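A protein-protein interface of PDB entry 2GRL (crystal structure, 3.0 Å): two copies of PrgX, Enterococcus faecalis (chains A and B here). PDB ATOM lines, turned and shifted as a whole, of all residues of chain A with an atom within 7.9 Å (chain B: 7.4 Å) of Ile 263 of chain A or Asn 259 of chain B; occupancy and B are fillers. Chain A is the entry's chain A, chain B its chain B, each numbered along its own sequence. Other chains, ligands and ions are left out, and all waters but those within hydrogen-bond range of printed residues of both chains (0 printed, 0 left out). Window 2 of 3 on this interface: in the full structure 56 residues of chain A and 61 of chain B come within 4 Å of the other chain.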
ATOM      1  N   TYR A 231      30.814  -8.101 -20.250  1.00  0.00           N
ATOM      2  CA  TYR A 231      29.385  -8.397 -20.113  1.00  0.00           C
ATOM      3  C   TYR A 231      29.130  -9.899 -20.148  1.00  0.00           C
ATOM      4  O   TYR A 231      28.269 -10.415 -19.420  1.00  0.00           O
ATOM      5  CB  TYR A 231      28.580  -7.715 -21.221  1.00  0.00           C
ATOM      6  CG  TYR A 231      28.645  -6.200 -21.221  1.00  0.00           C
ATOM      7  CD1 TYR A 231      28.117  -5.446 -20.169  1.00  0.00           C
ATOM      8  CD2 TYR A 231      29.241  -5.523 -22.274  1.00  0.00           C
ATOM      9  CE1 TYR A 231      28.186  -4.050 -20.172  1.00  0.00           C
ATOM     10  CE2 TYR A 231      29.318  -4.137 -22.299  1.00  0.00           C
ATOM     11  CZ  TYR A 231      28.793  -3.399 -21.250  1.00  0.00           C
ATOM     12  OH  TYR A 231      28.889  -2.016 -21.302  1.00  0.00           O
ATOM     13  N   LEU A 234      30.193 -11.425 -16.908  1.00  0.00           N
ATOM     14  CA  LEU A 234      29.156 -11.256 -15.889  1.00  0.00           C
ATOM     15  C   LEU A 234      28.038 -12.266 -16.062  1.00  0.00           C
ATOM     16  O   LEU A 234      27.690 -12.998 -15.129  1.00  0.00           O
ATOM     17  CB  LEU A 234      28.558  -9.847 -15.919  1.00  0.00           C
ATOM     18  CG  LEU A 234      29.357  -8.744 -15.235  1.00  0.00           C
ATOM     19  CD1 LEU A 234      28.625  -7.424 -15.324  1.00  0.00           C
ATOM     20  CD2 LEU A 234      29.566  -9.109 -13.791  1.00  0.00           C
ATOM     21  N   ASN A 256      24.425 -14.441  -4.954  1.00  0.00           N
ATOM     22  CA  ASN A 256      25.374 -13.856  -5.898  1.00  0.00           C
ATOM     23  C   ASN A 256      24.728 -13.662  -7.251  1.00  0.00           C
ATOM     24  O   ASN A 256      24.829 -12.593  -7.847  1.00  0.00           O
ATOM     25  CB  ASN A 256      26.583 -14.755  -6.096  1.00  0.00           C
ATOM     26  CG  ASN A 256      27.359 -14.956  -4.840  1.00  0.00           C
ATOM     27  OD1 ASN A 256      27.658 -14.001  -4.115  1.00  0.00           O
ATOM     28  ND2 ASN A 256      27.713 -16.206  -4.571  1.00  0.00           N
ATOM     29  N   ALA A 257      24.093 -14.721  -7.743  1.00  0.00           N
ATOM     30  CA  ALA A 257      23.445 -14.679  -9.042  1.00  0.00           C
ATOM     31  C   ALA A 257      22.531 -13.463  -9.094  1.00  0.00           C
ATOM     32  O   ALA A 257      22.512 -12.709 -10.085  1.00  0.00           O
ATOM     33  CB  ALA A 257      22.648 -15.948  -9.261  1.00  0.00           C
ATOM     34  N   VAL A 258      21.787 -13.262  -8.012  1.00  0.00           N
ATOM     35  CA  VAL A 258      20.874 -12.132  -7.935  1.00  0.00           C
ATOM     36  C   VAL A 258      21.624 -10.791  -7.915  1.00  0.00           C
ATOM     37  O   VAL A 258      21.148  -9.797  -8.474  1.00  0.00           O
ATOM     38  CB  VAL A 258      19.956 -12.265  -6.702  1.00  0.00           C
ATOM     39  CG1 VAL A 258      19.222 -10.983  -6.456  1.00  0.00           C
ATOM     40  CG2 VAL A 258      18.963 -13.384  -6.928  1.00  0.00           C
ATOM     41  N   ASN A 259      22.789 -10.759  -7.273  1.00  0.00           N
ATOM     42  CA  ASN A 259      23.590  -9.533  -7.239  1.00  0.00           C
ATOM     43  C   ASN A 259      24.030  -9.154  -8.658  1.00  0.00           C
ATOM     44  O   ASN A 259      23.971  -7.988  -9.045  1.00  0.00           O
ATOM     45  CB  ASN A 259      24.839  -9.720  -6.383  1.00  0.00           C
ATOM     46  CG  ASN A 259      24.554  -9.614  -4.922  1.00  0.00           C
ATOM     47  OD1 ASN A 259      23.949  -8.641  -4.475  1.00  0.00           O
ATOM     48  ND2 ASN A 259      25.000 -10.607  -4.153  1.00  0.00           N
ATOM     49  N   ILE A 260      24.488 -10.148  -9.417  1.00  0.00           N
ATOM     50  CA  ILE A 260      24.934  -9.934 -10.785  1.00  0.00           C
ATOM     51  C   ILE A 260      23.768  -9.392 -11.597  1.00  0.00           C
ATOM     52  O   ILE A 260      23.891  -8.365 -12.282  1.00  0.00           O
ATOM     53  CB  ILE A 260      25.436 -11.247 -11.408  1.00  0.00           C
ATOM     54  CG1 ILE A 260      26.674 -11.720 -10.651  1.00  0.00           C
ATOM     55  CG2 ILE A 260      25.747 -11.058 -12.883  1.00  0.00           C
ATOM     56  CD1 ILE A 260      27.187 -13.084 -11.098  1.00  0.00           C
ATOM     57  N   ILE A 261      22.630 -10.073 -11.515  1.00  0.00           N
ATOM     58  CA  ILE A 261      21.454  -9.610 -12.235  1.00  0.00           C
ATOM     59  C   ILE A 261      21.205  -8.140 -11.893  1.00  0.00           C
ATOM     60  O   ILE A 261      20.937  -7.320 -12.770  1.00  0.00           O
ATOM     61  CB  ILE A 261      20.211 -10.458 -11.881  1.00  0.00           C
ATOM     62  CG1 ILE A 261      20.398 -11.872 -12.438  1.00  0.00           C
ATOM     63  CG2 ILE A 261      18.952  -9.822 -12.452  1.00  0.00           C
ATOM     64  CD1 ILE A 261      19.186 -12.776 -12.301  1.00  0.00           C
ATOM     65  N   ASN A 262      21.313  -7.804 -10.613  1.00  0.00           N
ATOM     66  CA  ASN A 262      21.123  -6.425 -10.181  1.00  0.00           C
ATOM     67  C   ASN A 262      22.106  -5.467 -10.889  1.00  0.00           C
ATOM     68  O   ASN A 262      21.709  -4.452 -11.450  1.00  0.00           O
ATOM     69  CB  ASN A 262      21.319  -6.326  -8.669  1.00  0.00           C
ATOM     70  CG  ASN A 262      20.847  -4.997  -8.105  1.00  0.00           C
ATOM     71  OD1 ASN A 262      21.517  -4.387  -7.265  1.00  0.00           O
ATOM     72  ND2 ASN A 262      19.680  -4.548  -8.556  1.00  0.00           N
ATOM     73  N   ILE A 263      23.391  -5.805 -10.850  1.00  0.00           N
ATOM     74  CA  ILE A 263      24.433  -4.999 -11.464  1.00  0.00           C
ATOM     75  C   ILE A 263      24.120  -4.573 -12.895  1.00  0.00           C
ATOM     76  O   ILE A 263      24.392  -3.429 -13.280  1.00  0.00           O
ATOM     77  CB  ILE A 263      25.781  -5.751 -11.405  1.00  0.00           C
ATOM     78  CG1 ILE A 263      26.419  -5.492 -10.046  1.00  0.00           C
ATOM     79  CG2 ILE A 263      26.701  -5.317 -12.528  1.00  0.00           C
ATOM     80  CD1 ILE A 263      26.609  -4.034  -9.732  1.00  0.00           C
ATOM     81  N   PHE A 264      23.557  -5.487 -13.682  1.00  0.00           N
ATOM     82  CA  PHE A 264      23.204  -5.176 -15.069  1.00  0.00           C
ATOM     83  C   PHE A 264      22.223  -4.020 -15.092  1.00  0.00           C
ATOM     84  O   PHE A 264      22.357  -3.090 -15.887  1.00  0.00           O
ATOM     85  CB  PHE A 264      22.602  -6.401 -15.781  1.00  0.00           C
ATOM     86  CG  PHE A 264      23.637  -7.317 -16.383  1.00  0.00           C
ATOM     87  CD1 PHE A 264      24.398  -6.905 -17.475  1.00  0.00           C
ATOM     88  CD2 PHE A 264      23.897  -8.568 -15.828  1.00  0.00           C
ATOM     89  CE1 PHE A 264      25.409  -7.731 -18.001  1.00  0.00           C
ATOM     90  CE2 PHE A 264      24.902  -9.395 -16.346  1.00  0.00           C
ATOM     91  CZ  PHE A 264      25.656  -8.978 -17.428  1.00  0.00           C
ATOM     92  N   LYS A 265      21.236  -4.083 -14.210  1.00  0.00           N
ATOM     93  CA  LYS A 265      20.255  -3.011 -14.097  1.00  0.00           C
ATOM     94  C   LYS A 265      20.970  -1.721 -13.670  1.00  0.00           C
ATOM     95  O   LYS A 265      20.699  -0.657 -14.209  1.00  0.00           O
ATOM     96  CB  LYS A 265      19.200  -3.367 -13.054  1.00  0.00           C
ATOM     97  CG  LYS A 265      18.213  -2.262 -12.775  1.00  0.00           C
ATOM     98  CD  LYS A 265      17.383  -2.574 -11.544  1.00  0.00           C
ATOM     99  CE  LYS A 265      16.373  -1.475 -11.272  1.00  0.00           C
ATOM    100  NZ  LYS A 265      15.604  -1.731 -10.024  1.00  0.00           N
ATOM    101  N   ILE A 266      21.888  -1.823 -12.714  1.00  0.00           N
ATOM    102  CA  ILE A 266      22.614  -0.663 -12.237  1.00  0.00           C
ATOM    103  C   ILE A 266      23.435   0.045 -13.306  1.00  0.00           C
ATOM    104  O   ILE A 266      23.361   1.272 -13.412  1.00  0.00           O
ATOM    105  CB  ILE A 266      23.552  -1.024 -11.085  1.00  0.00           C
ATOM    106  CG1 ILE A 266      22.731  -1.410  -9.864  1.00  0.00           C
ATOM    107  CG2 ILE A 266      24.445   0.155 -10.747  1.00  0.00           C
ATOM    108  CD1 ILE A 266      23.564  -1.679  -8.605  1.00  0.00           C
ATOM    109  N   ILE A 267      24.221  -0.704 -14.082  1.00  0.00           N
ATOM    110  CA  ILE A 267      25.060  -0.094 -15.117  1.00  0.00           C
ATOM    111  C   ILE A 267      24.275   0.257 -16.361  1.00  0.00           C
ATOM    112  O   ILE A 267      24.834   0.755 -17.349  1.00  0.00           O
ATOM    113  CB  ILE A 267      26.226  -0.998 -15.541  1.00  0.00           C
ATOM    114  CG1 ILE A 267      25.683  -2.294 -16.129  1.00  0.00           C
ATOM    115  CG2 ILE A 267      27.150  -1.238 -14.368  1.00  0.00           C
ATOM    116  CD1 ILE A 267      26.755  -3.201 -16.627  1.00  0.00           C
ATOM    117  N   GLY A 268      22.980  -0.037 -16.323  1.00  0.00           N
ATOM    118  CA  GLY A 268      22.121   0.311 -17.438  1.00  0.00           C
ATOM    119  C   GLY A 268      21.835  -0.700 -18.541  1.00  0.00           C
ATOM    120  O   GLY A 268      21.090  -0.396 -19.490  1.00  0.00           O
ATOM    121  N   LYS A 269      22.408  -1.897 -18.453  1.00  0.00           N
ATOM    122  CA  LYS A 269      22.157  -2.895 -19.494  1.00  0.00           C
ATOM    123  C   LYS A 269      20.762  -3.476 -19.292  1.00  0.00           C
ATOM    124  O   LYS A 269      20.601  -4.650 -18.973  1.00  0.00           O
ATOM    125  CB  LYS A 269      23.224  -3.988 -19.440  1.00  0.00           C
ATOM    126  CG  LYS A 269      24.648  -3.457 -19.616  1.00  0.00           C
ATOM    127  CD  LYS A 269      24.905  -2.890 -21.014  1.00  0.00           C
ATOM    128  CE  LYS A 269      24.916  -3.991 -22.066  1.00  0.00           C
ATOM    129  NZ  LYS A 269      25.359  -3.514 -23.405  1.00  0.00           N
ATOM    130  N   GLU A 270      19.759  -2.623 -19.492  1.00  0.00           N
ATOM    131  CA  GLU A 270      18.349  -2.970 -19.315  1.00  0.00           C
ATOM    132  C   GLU A 270      17.884  -4.242 -20.025  1.00  0.00           C
ATOM    133  O   GLU A 270      17.261  -5.106 -19.417  1.00  0.00           O
ATOM    134  CB  GLU A 270      17.469  -1.796 -19.746  1.00  0.00           C
ATOM    135  CG  GLU A 270      16.017  -1.918 -19.316  1.00  0.00           C
ATOM    136  CD  GLU A 270      15.862  -2.042 -17.806  1.00  0.00           C
ATOM    137  OE1 GLU A 270      16.402  -1.177 -17.082  1.00  0.00           O
ATOM    138  OE2 GLU A 270      15.199  -2.999 -17.345  1.00  0.00           O
ATOM    139  N   HIS A 273      19.267  -7.129 -18.379  1.00  0.00           N
ATOM    140  CA  HIS A 273      18.602  -7.221 -17.085  1.00  0.00           C
ATOM    141  C   HIS A 273      17.283  -7.974 -17.193  1.00  0.00           C
ATOM    142  O   HIS A 273      17.092  -9.004 -16.539  1.00  0.00           O
ATOM    143  CB  HIS A 273      18.339  -5.836 -16.495  1.00  0.00           C
ATOM    144  CG  HIS A 273      17.748  -5.881 -15.119  1.00  0.00           C
ATOM    145  ND1 HIS A 273      16.596  -5.208 -14.780  1.00  0.00           N
ATOM    146  CD2 HIS A 273      18.147  -6.536 -14.002  1.00  0.00           C
ATOM    147  CE1 HIS A 273      16.310  -5.446 -13.513  1.00  0.00           C
ATOM    148  NE2 HIS A 273      17.234  -6.248 -13.019  1.00  0.00           N
ATOM    149  N   LEU B 234      31.215  -1.162 -16.078  1.00  0.00           N
ATOM    150  CA  LEU B 234      31.017  -1.389 -14.652  1.00  0.00           C
ATOM    151  C   LEU B 234      31.781  -0.369 -13.830  1.00  0.00           C
ATOM    152  O   LEU B 234      31.199   0.320 -13.003  1.00  0.00           O
ATOM    153  CB  LEU B 234      31.471  -2.796 -14.244  1.00  0.00           C
ATOM    154  CG  LEU B 234      30.509  -3.944 -14.529  1.00  0.00           C
ATOM    155  CD1 LEU B 234      31.105  -5.243 -14.042  1.00  0.00           C
ATOM    156  CD2 LEU B 234      29.207  -3.692 -13.837  1.00  0.00           C
ATOM    157  N   ASN B 237      30.572   3.106 -14.180  1.00  0.00           N
ATOM    158  CA  ASN B 237      29.267   3.215 -13.533  1.00  0.00           C
ATOM    159  C   ASN B 237      29.396   3.290 -12.031  1.00  0.00           C
ATOM    160  O   ASN B 237      28.561   3.882 -11.364  1.00  0.00           O
ATOM    161  CB  ASN B 237      28.361   2.054 -13.936  1.00  0.00           C
ATOM    162  CG  ASN B 237      27.101   2.536 -14.614  1.00  0.00           C
ATOM    163  OD1 ASN B 237      26.164   2.992 -13.950  1.00  0.00           O
ATOM    164  ND2 ASN B 237      27.076   2.474 -15.946  1.00  0.00           N
ATOM    165  N   TYR B 238      30.451   2.697 -11.495  1.00  0.00           N
ATOM    166  CA  TYR B 238      30.670   2.754 -10.058  1.00  0.00           C
ATOM    167  C   TYR B 238      31.140   4.170  -9.722  1.00  0.00           C
ATOM    168  O   TYR B 238      30.816   4.718  -8.667  1.00  0.00           O
ATOM    169  CB  TYR B 238      31.703   1.708  -9.623  1.00  0.00           C
ATOM    170  CG  TYR B 238      32.716   2.205  -8.627  1.00  0.00           C
ATOM    171  CD1 TYR B 238      33.857   2.881  -9.049  1.00  0.00           C
ATOM    172  CD2 TYR B 238      32.516   2.034  -7.261  1.00  0.00           C
ATOM    173  CE1 TYR B 238      34.776   3.374  -8.136  1.00  0.00           C
ATOM    174  CE2 TYR B 238      33.427   2.529  -6.333  1.00  0.00           C
ATOM    175  CZ  TYR B 238      34.555   3.196  -6.779  1.00  0.00           C
ATOM    176  OH  TYR B 238      35.474   3.686  -5.879  1.00  0.00           O
ATOM    177  N   ASP B 252      21.580   5.462  -1.309  1.00  0.00           N
ATOM    178  CA  ASP B 252      21.387   4.413  -2.310  1.00  0.00           C
ATOM    179  C   ASP B 252      22.576   4.313  -3.266  1.00  0.00           C
ATOM    180  O   ASP B 252      22.983   3.212  -3.644  1.00  0.00           O
ATOM    181  CB  ASP B 252      20.113   4.679  -3.118  1.00  0.00           C
ATOM    182  CG  ASP B 252      18.866   4.627  -2.268  1.00  0.00           C
ATOM    183  OD1 ASP B 252      18.514   3.521  -1.805  1.00  0.00           O
ATOM    184  OD2 ASP B 252      18.246   5.691  -2.057  1.00  0.00           O
ATOM    185  N   SER B 253      23.124   5.466  -3.658  1.00  0.00           N
ATOM    186  CA  SER B 253      24.261   5.510  -4.574  1.00  0.00           C
ATOM    187  C   SER B 253      25.443   4.754  -3.976  1.00  0.00           C
ATOM    188  O   SER B 253      26.013   3.854  -4.605  1.00  0.00           O
ATOM    189  CB  SER B 253      24.646   6.968  -4.863  1.00  0.00           C
ATOM    190  OG  SER B 253      23.656   7.608  -5.654  1.00  0.00           O
ATOM    191  N   TYR B 254      25.796   5.128  -2.750  1.00  0.00           N
ATOM    192  CA  TYR B 254      26.897   4.491  -2.038  1.00  0.00           C
ATOM    193  C   TYR B 254      26.713   2.972  -2.034  1.00  0.00           C
ATOM    194  O   TYR B 254      27.666   2.222  -2.207  1.00  0.00           O
ATOM    195  CB  TYR B 254      26.967   5.015  -0.602  1.00  0.00           C
ATOM    196  CG  TYR B 254      28.260   4.660   0.091  1.00  0.00           C
ATOM    197  CD1 TYR B 254      28.433   3.430   0.712  1.00  0.00           C
ATOM    198  CD2 TYR B 254      29.336   5.535   0.059  1.00  0.00           C
ATOM    199  CE1 TYR B 254      29.647   3.087   1.277  1.00  0.00           C
ATOM    200  CE2 TYR B 254      30.551   5.201   0.612  1.00  0.00           C
ATOM    201  CZ  TYR B 254      30.706   3.983   1.216  1.00  0.00           C
ATOM    202  OH  TYR B 254      31.944   3.668   1.731  1.00  0.00           O
ATOM    203  N   LEU B 255      25.471   2.536  -1.836  1.00  0.00           N
ATOM    204  CA  LEU B 255      25.117   1.123  -1.822  1.00  0.00           C
ATOM    205  C   LEU B 255      25.410   0.491  -3.188  1.00  0.00           C
ATOM    206  O   LEU B 255      26.096  -0.529  -3.265  1.00  0.00           O
ATOM    207  CB  LEU B 255      23.635   0.975  -1.460  1.00  0.00           C
ATOM    208  CG  LEU B 255      23.248   1.038   0.027  1.00  0.00           C
ATOM    209  CD1 LEU B 255      23.786  -0.180   0.738  1.00  0.00           C
ATOM    210  CD2 LEU B 255      23.787   2.291   0.681  1.00  0.00           C
ATOM    211  N   ASN B 256      24.903   1.102  -4.261  1.00  0.00           N
ATOM    212  CA  ASN B 256      25.129   0.585  -5.607  1.00  0.00           C
ATOM    213  C   ASN B 256      26.603   0.487  -5.890  1.00  0.00           C
ATOM    214  O   ASN B 256      27.091  -0.534  -6.363  1.00  0.00           O
ATOM    215  CB  ASN B 256      24.520   1.489  -6.669  1.00  0.00           C
ATOM    216  CG  ASN B 256      23.051   1.628  -6.525  1.00  0.00           C
ATOM    217  OD1 ASN B 256      22.337   0.639  -6.342  1.00  0.00           O
ATOM    218  ND2 ASN B 256      22.570   2.860  -6.610  1.00  0.00           N
ATOM    219  N   ALA B 257      27.314   1.568  -5.615  1.00  0.00           N
ATOM    220  CA  ALA B 257      28.745   1.593  -5.864  1.00  0.00           C
ATOM    221  C   ALA B 257      29.395   0.382  -5.213  1.00  0.00           C
ATOM    222  O   ALA B 257      30.239  -0.292  -5.814  1.00  0.00           O
ATOM    223  CB  ALA B 257      29.351   2.877  -5.313  1.00  0.00           C
ATOM    224  N   VAL B 258      28.995   0.106  -3.980  1.00  0.00           N
ATOM    225  CA  VAL B 258      29.537  -1.029  -3.250  1.00  0.00           C
ATOM    226  C   VAL B 258      29.135  -2.369  -3.897  1.00  0.00           C
ATOM    227  O   VAL B 258      29.917  -3.318  -3.898  1.00  0.00           O
ATOM    228  CB  VAL B 258      29.080  -0.971  -1.797  1.00  0.00           C
ATOM    229  CG1 VAL B 258      29.387  -2.261  -1.100  1.00  0.00           C
ATOM    230  CG2 VAL B 258      29.778   0.174  -1.094  1.00  0.00           C
ATOM    231  N   ASN B 259      27.925  -2.446  -4.446  1.00  0.00           N
ATOM    232  CA  ASN B 259      27.479  -3.667  -5.113  1.00  0.00           C
ATOM    233  C   ASN B 259      28.368  -3.952  -6.327  1.00  0.00           C
ATOM    234  O   ASN B 259      28.750  -5.099  -6.575  1.00  0.00           O
ATOM    235  CB  ASN B 259      26.036  -3.528  -5.603  1.00  0.00           C
ATOM    236  CG  ASN B 259      25.030  -3.739  -4.510  1.00  0.00           C
ATOM    237  OD1 ASN B 259      25.094  -4.740  -3.795  1.00  0.00           O
ATOM    238  ND2 ASN B 259      24.076  -2.803  -4.380  1.00  0.00           N
ATOM    239  N   ILE B 260      28.668  -2.904  -7.095  1.00  0.00           N
ATOM    240  CA  ILE B 260      29.503  -3.033  -8.286  1.00  0.00           C
ATOM    241  C   ILE B 260      30.877  -3.533  -7.869  1.00  0.00           C
ATOM    242  O   ILE B 260      31.390  -4.516  -8.415  1.00  0.00           O
ATOM    243  CB  ILE B 260      29.638  -1.680  -9.006  1.00  0.00           C
ATOM    244  CG1 ILE B 260      28.270  -1.246  -9.534  1.00  0.00           C
ATOM    245  CG2 ILE B 260      30.632  -1.783 -10.145  1.00  0.00           C
ATOM    246  CD1 ILE B 260      28.265   0.119 -10.173  1.00  0.00           C
ATOM    247  N   ILE B 261      31.477  -2.855  -6.894  1.00  0.00           N
ATOM    248  CA  ILE B 261      32.773  -3.276  -6.397  1.00  0.00           C
ATOM    249  C   ILE B 261      32.689  -4.764  -6.057  1.00  0.00           C
ATOM    250  O   ILE B 261      33.570  -5.533  -6.420  1.00  0.00           O
ATOM    251  CB  ILE B 261      33.182  -2.459  -5.153  1.00  0.00           C
ATOM    252  CG1 ILE B 261      33.445  -1.011  -5.577  1.00  0.00           C
ATOM    253  CG2 ILE B 261      34.417  -3.056  -4.501  1.00  0.00           C
ATOM    254  CD1 ILE B 261      34.010  -0.113  -4.476  1.00  0.00           C
ATOM    255  N   ASN B 262      31.613  -5.168  -5.388  1.00  0.00           N
ATOM    256  CA  ASN B 262      31.441  -6.566  -5.024  1.00  0.00           C
ATOM    257  C   ASN B 262      31.461  -7.474  -6.259  1.00  0.00           C
ATOM    258  O   ASN B 262      32.173  -8.471  -6.300  1.00  0.00           O
ATOM    259  CB  ASN B 262      30.120  -6.761  -4.281  1.00  0.00           C
ATOM    260  CG  ASN B 262      30.015  -8.129  -3.634  1.00  0.00           C
ATOM    261  OD1 ASN B 262      28.970  -8.781  -3.703  1.00  0.00           O
ATOM    262  ND2 ASN B 262      31.100  -8.566  -2.989  1.00  0.00           N
ATOM    263  N   ILE B 263      30.663  -7.126  -7.259  1.00  0.00           N
ATOM    264  CA  ILE B 263      30.576  -7.909  -8.483  1.00  0.00           C
ATOM    265  C   ILE B 263      31.930  -8.247  -9.093  1.00  0.00           C
ATOM    266  O   ILE B 263      32.136  -9.363  -9.578  1.00  0.00           O
ATOM    267  CB  ILE B 263      29.698  -7.178  -9.507  1.00  0.00           C
ATOM    268  CG1 ILE B 263      28.250  -7.540  -9.235  1.00  0.00           C
ATOM    269  CG2 ILE B 263      30.083  -7.542 -10.923  1.00  0.00           C
ATOM    270  CD1 ILE B 263      27.980  -9.017  -9.276  1.00  0.00           C
ATOM    271  N   PHE B 264      32.852  -7.289  -9.078  1.00  0.00           N
ATOM    272  CA  PHE B 264      34.182  -7.532  -9.629  1.00  0.00           C
ATOM    273  C   PHE B 264      34.842  -8.689  -8.889  1.00  0.00           C
ATOM    274  O   PHE B 264      35.448  -9.568  -9.504  1.00  0.00           O
ATOM    275  CB  PHE B 264      35.040  -6.275  -9.530  1.00  0.00           C
ATOM    276  CG  PHE B 264      34.848  -5.337 -10.677  1.00  0.00           C
ATOM    277  CD1 PHE B 264      35.296  -5.680 -11.947  1.00  0.00           C
ATOM    278  CD2 PHE B 264      34.185  -4.126 -10.505  1.00  0.00           C
ATOM    279  CE1 PHE B 264      35.086  -4.829 -13.038  1.00  0.00           C
ATOM    280  CE2 PHE B 264      33.967  -3.264 -11.592  1.00  0.00           C
ATOM    281  CZ  PHE B 264      34.418  -3.617 -12.858  1.00  0.00           C
ATOM    282  N   LYS B 265      34.720  -8.681  -7.565  1.00  0.00           N
ATOM    283  CA  LYS B 265      35.270  -9.753  -6.749  1.00  0.00           C
ATOM    284  C   LYS B 265      34.579 -11.057  -7.132  1.00  0.00           C
ATOM    285  O   LYS B 265      35.223 -12.078  -7.283  1.00  0.00           O
ATOM    286  CB  LYS B 265      35.034  -9.464  -5.266  1.00  0.00           C
ATOM    287  CG  LYS B 265      35.435 -10.598  -4.339  1.00  0.00           C
ATOM    288  CD  LYS B 265      34.934 -10.350  -2.919  1.00  0.00           C
ATOM    289  CE  LYS B 265      35.379 -11.461  -1.989  1.00  0.00           C
ATOM    290  NZ  LYS B 265      34.844 -11.275  -0.624  1.00  0.00           N
ATOM    291  N   ILE B 266      33.264 -11.012  -7.309  1.00  0.00           N
ATOM    292  CA  ILE B 266      32.500 -12.203  -7.647  1.00  0.00           C
ATOM    293  C   ILE B 266      32.901 -12.858  -8.965  1.00  0.00           C
ATOM    294  O   ILE B 266      33.084 -14.076  -9.024  1.00  0.00           O
ATOM    295  CB  ILE B 266      30.983 -11.907  -7.696  1.00  0.00           C
ATOM    296  CG1 ILE B 266      30.472 -11.589  -6.293  1.00  0.00           C
ATOM    297  CG2 ILE B 266      30.233 -13.102  -8.275  1.00  0.00           C
ATOM    298  CD1 ILE B 266      28.954 -11.376  -6.225  1.00  0.00           C
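The backbone carbonyl oxygen of Asp 252 of chain B lies within hydrogen-bond range of the side-chain amide nitrogen of Asn 256 of chain B (3.0 Å). O of Leu 255 of chain B lies within hydrogen-bond range of ND2 of Asn 259 of chain B (3.2 Å).
Ile 263 of chain A touches just these residues of chain B: Leu 234, Asn 259, Ile 260 and Ile 263. Of chain A, only Ile 263 comes within 4 Å of Asn 259 of chain B. Of the printed residues of chain B, Asn 256 of chain A touches Ile 266 (3.6 Å). Of the printed residues of chain A, Ile 266 of chain B touches Asn 256. Of the printed residues of chain B, Ile 266 of chain A touches Asn 237 (3.3 Å), Asn 256 (3.5 Å) and Ile 260 (3.9 Å). Printed residues of chain A within 4 Å of Asn 237 of chain B: Ile 266 (3.3 Å) and Ile 267 (3.2 Å). Printed residues of chain B within 4 Å of Ile 260 of chain A: Ile 263. The nearest residue of chain B that does not touch Ile 263 of chain A is Asn 256 of chain B (4.9 Å). The nearest residue of chain A that does not touch Asn 259 of chain B is Asn 259 of chain A (4.1 Å).
Leu 234 of chain B touches its own counterpart, Leu 234 of chain A. Asn 256 of chain A touches Ile 266 of chain B, and with the chains exchanged Ile 266 of chain A touches Asn 256 of chain B. Ile 260 of chain A touches Ile 263 of chain B, and with the chains exchanged Ile 263 of chain A touches Ile 260 of chain B. Ile 266 of chain A touches Ile 260 of chain B, but with the chains exchanged Ile 260 of chain A does not touch Ile 266 of chain B (4.2 Å). Positions printed for both chains: 234, 256, 257, 258, 259, 260, 261, 262, 263, 264, 265 and 266. Of the 13 pairs that touch across the chains among the printed residues, 8 have their exchanged pair printed and touching as well.
O of Ile 266 of chain A sits close to OD1 of Asn 237 of chain B, at 3.3 Å. ND2 of Asn 237 of chain B sits at hydrogen-bond distance from O of Ile 267 of chain A, 3.2 Å away.
Leu 234 of chain A touches Leu 234 of chain B. CG2 of Ile 263 of chain B touches CD2 of Leu 234 of chain A, 3.3 Å away. Ile 266 of chain B touches Asn 256 of chain A. Ile 260 of chain A touches Ile 263 of chain B (CG1 to CD1, 3.3 Å). Ile 263 of chain A touches Leu 234 of chain B (CG2 to CD2, 3.3 Å). CD1 of Ile 263 of chain A touches CG1 of Ile 260 of chain B, 3.3 Å away. CG1 of Ile 263 of chain B touches CG1 of Ile 263 of chain A, at 2.9 Å. CD1 of Ile 266 of chain A touches OD1 of Asn 256 of chain B (3.5 Å). CG2 of Ile 266 of chain A touches CD1 of Ile 260 of chain B, 3.9 Å away. Leu 234 of chain B touches Ile 267 of chain A.
Of the 18 printed residues of chain B, 7 touch a printed residue of chain A. Printed residues of chain B that touch a printed residue of chain A: Leu 234, Asn 237, Asn 256, Asn 259, Ile 260, Ile 263 and Ile 266. Of the 18 printed residues of chain A, 6 touch a printed residue of chain B. Among the printed residues, 13 pairs touch across the chains.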
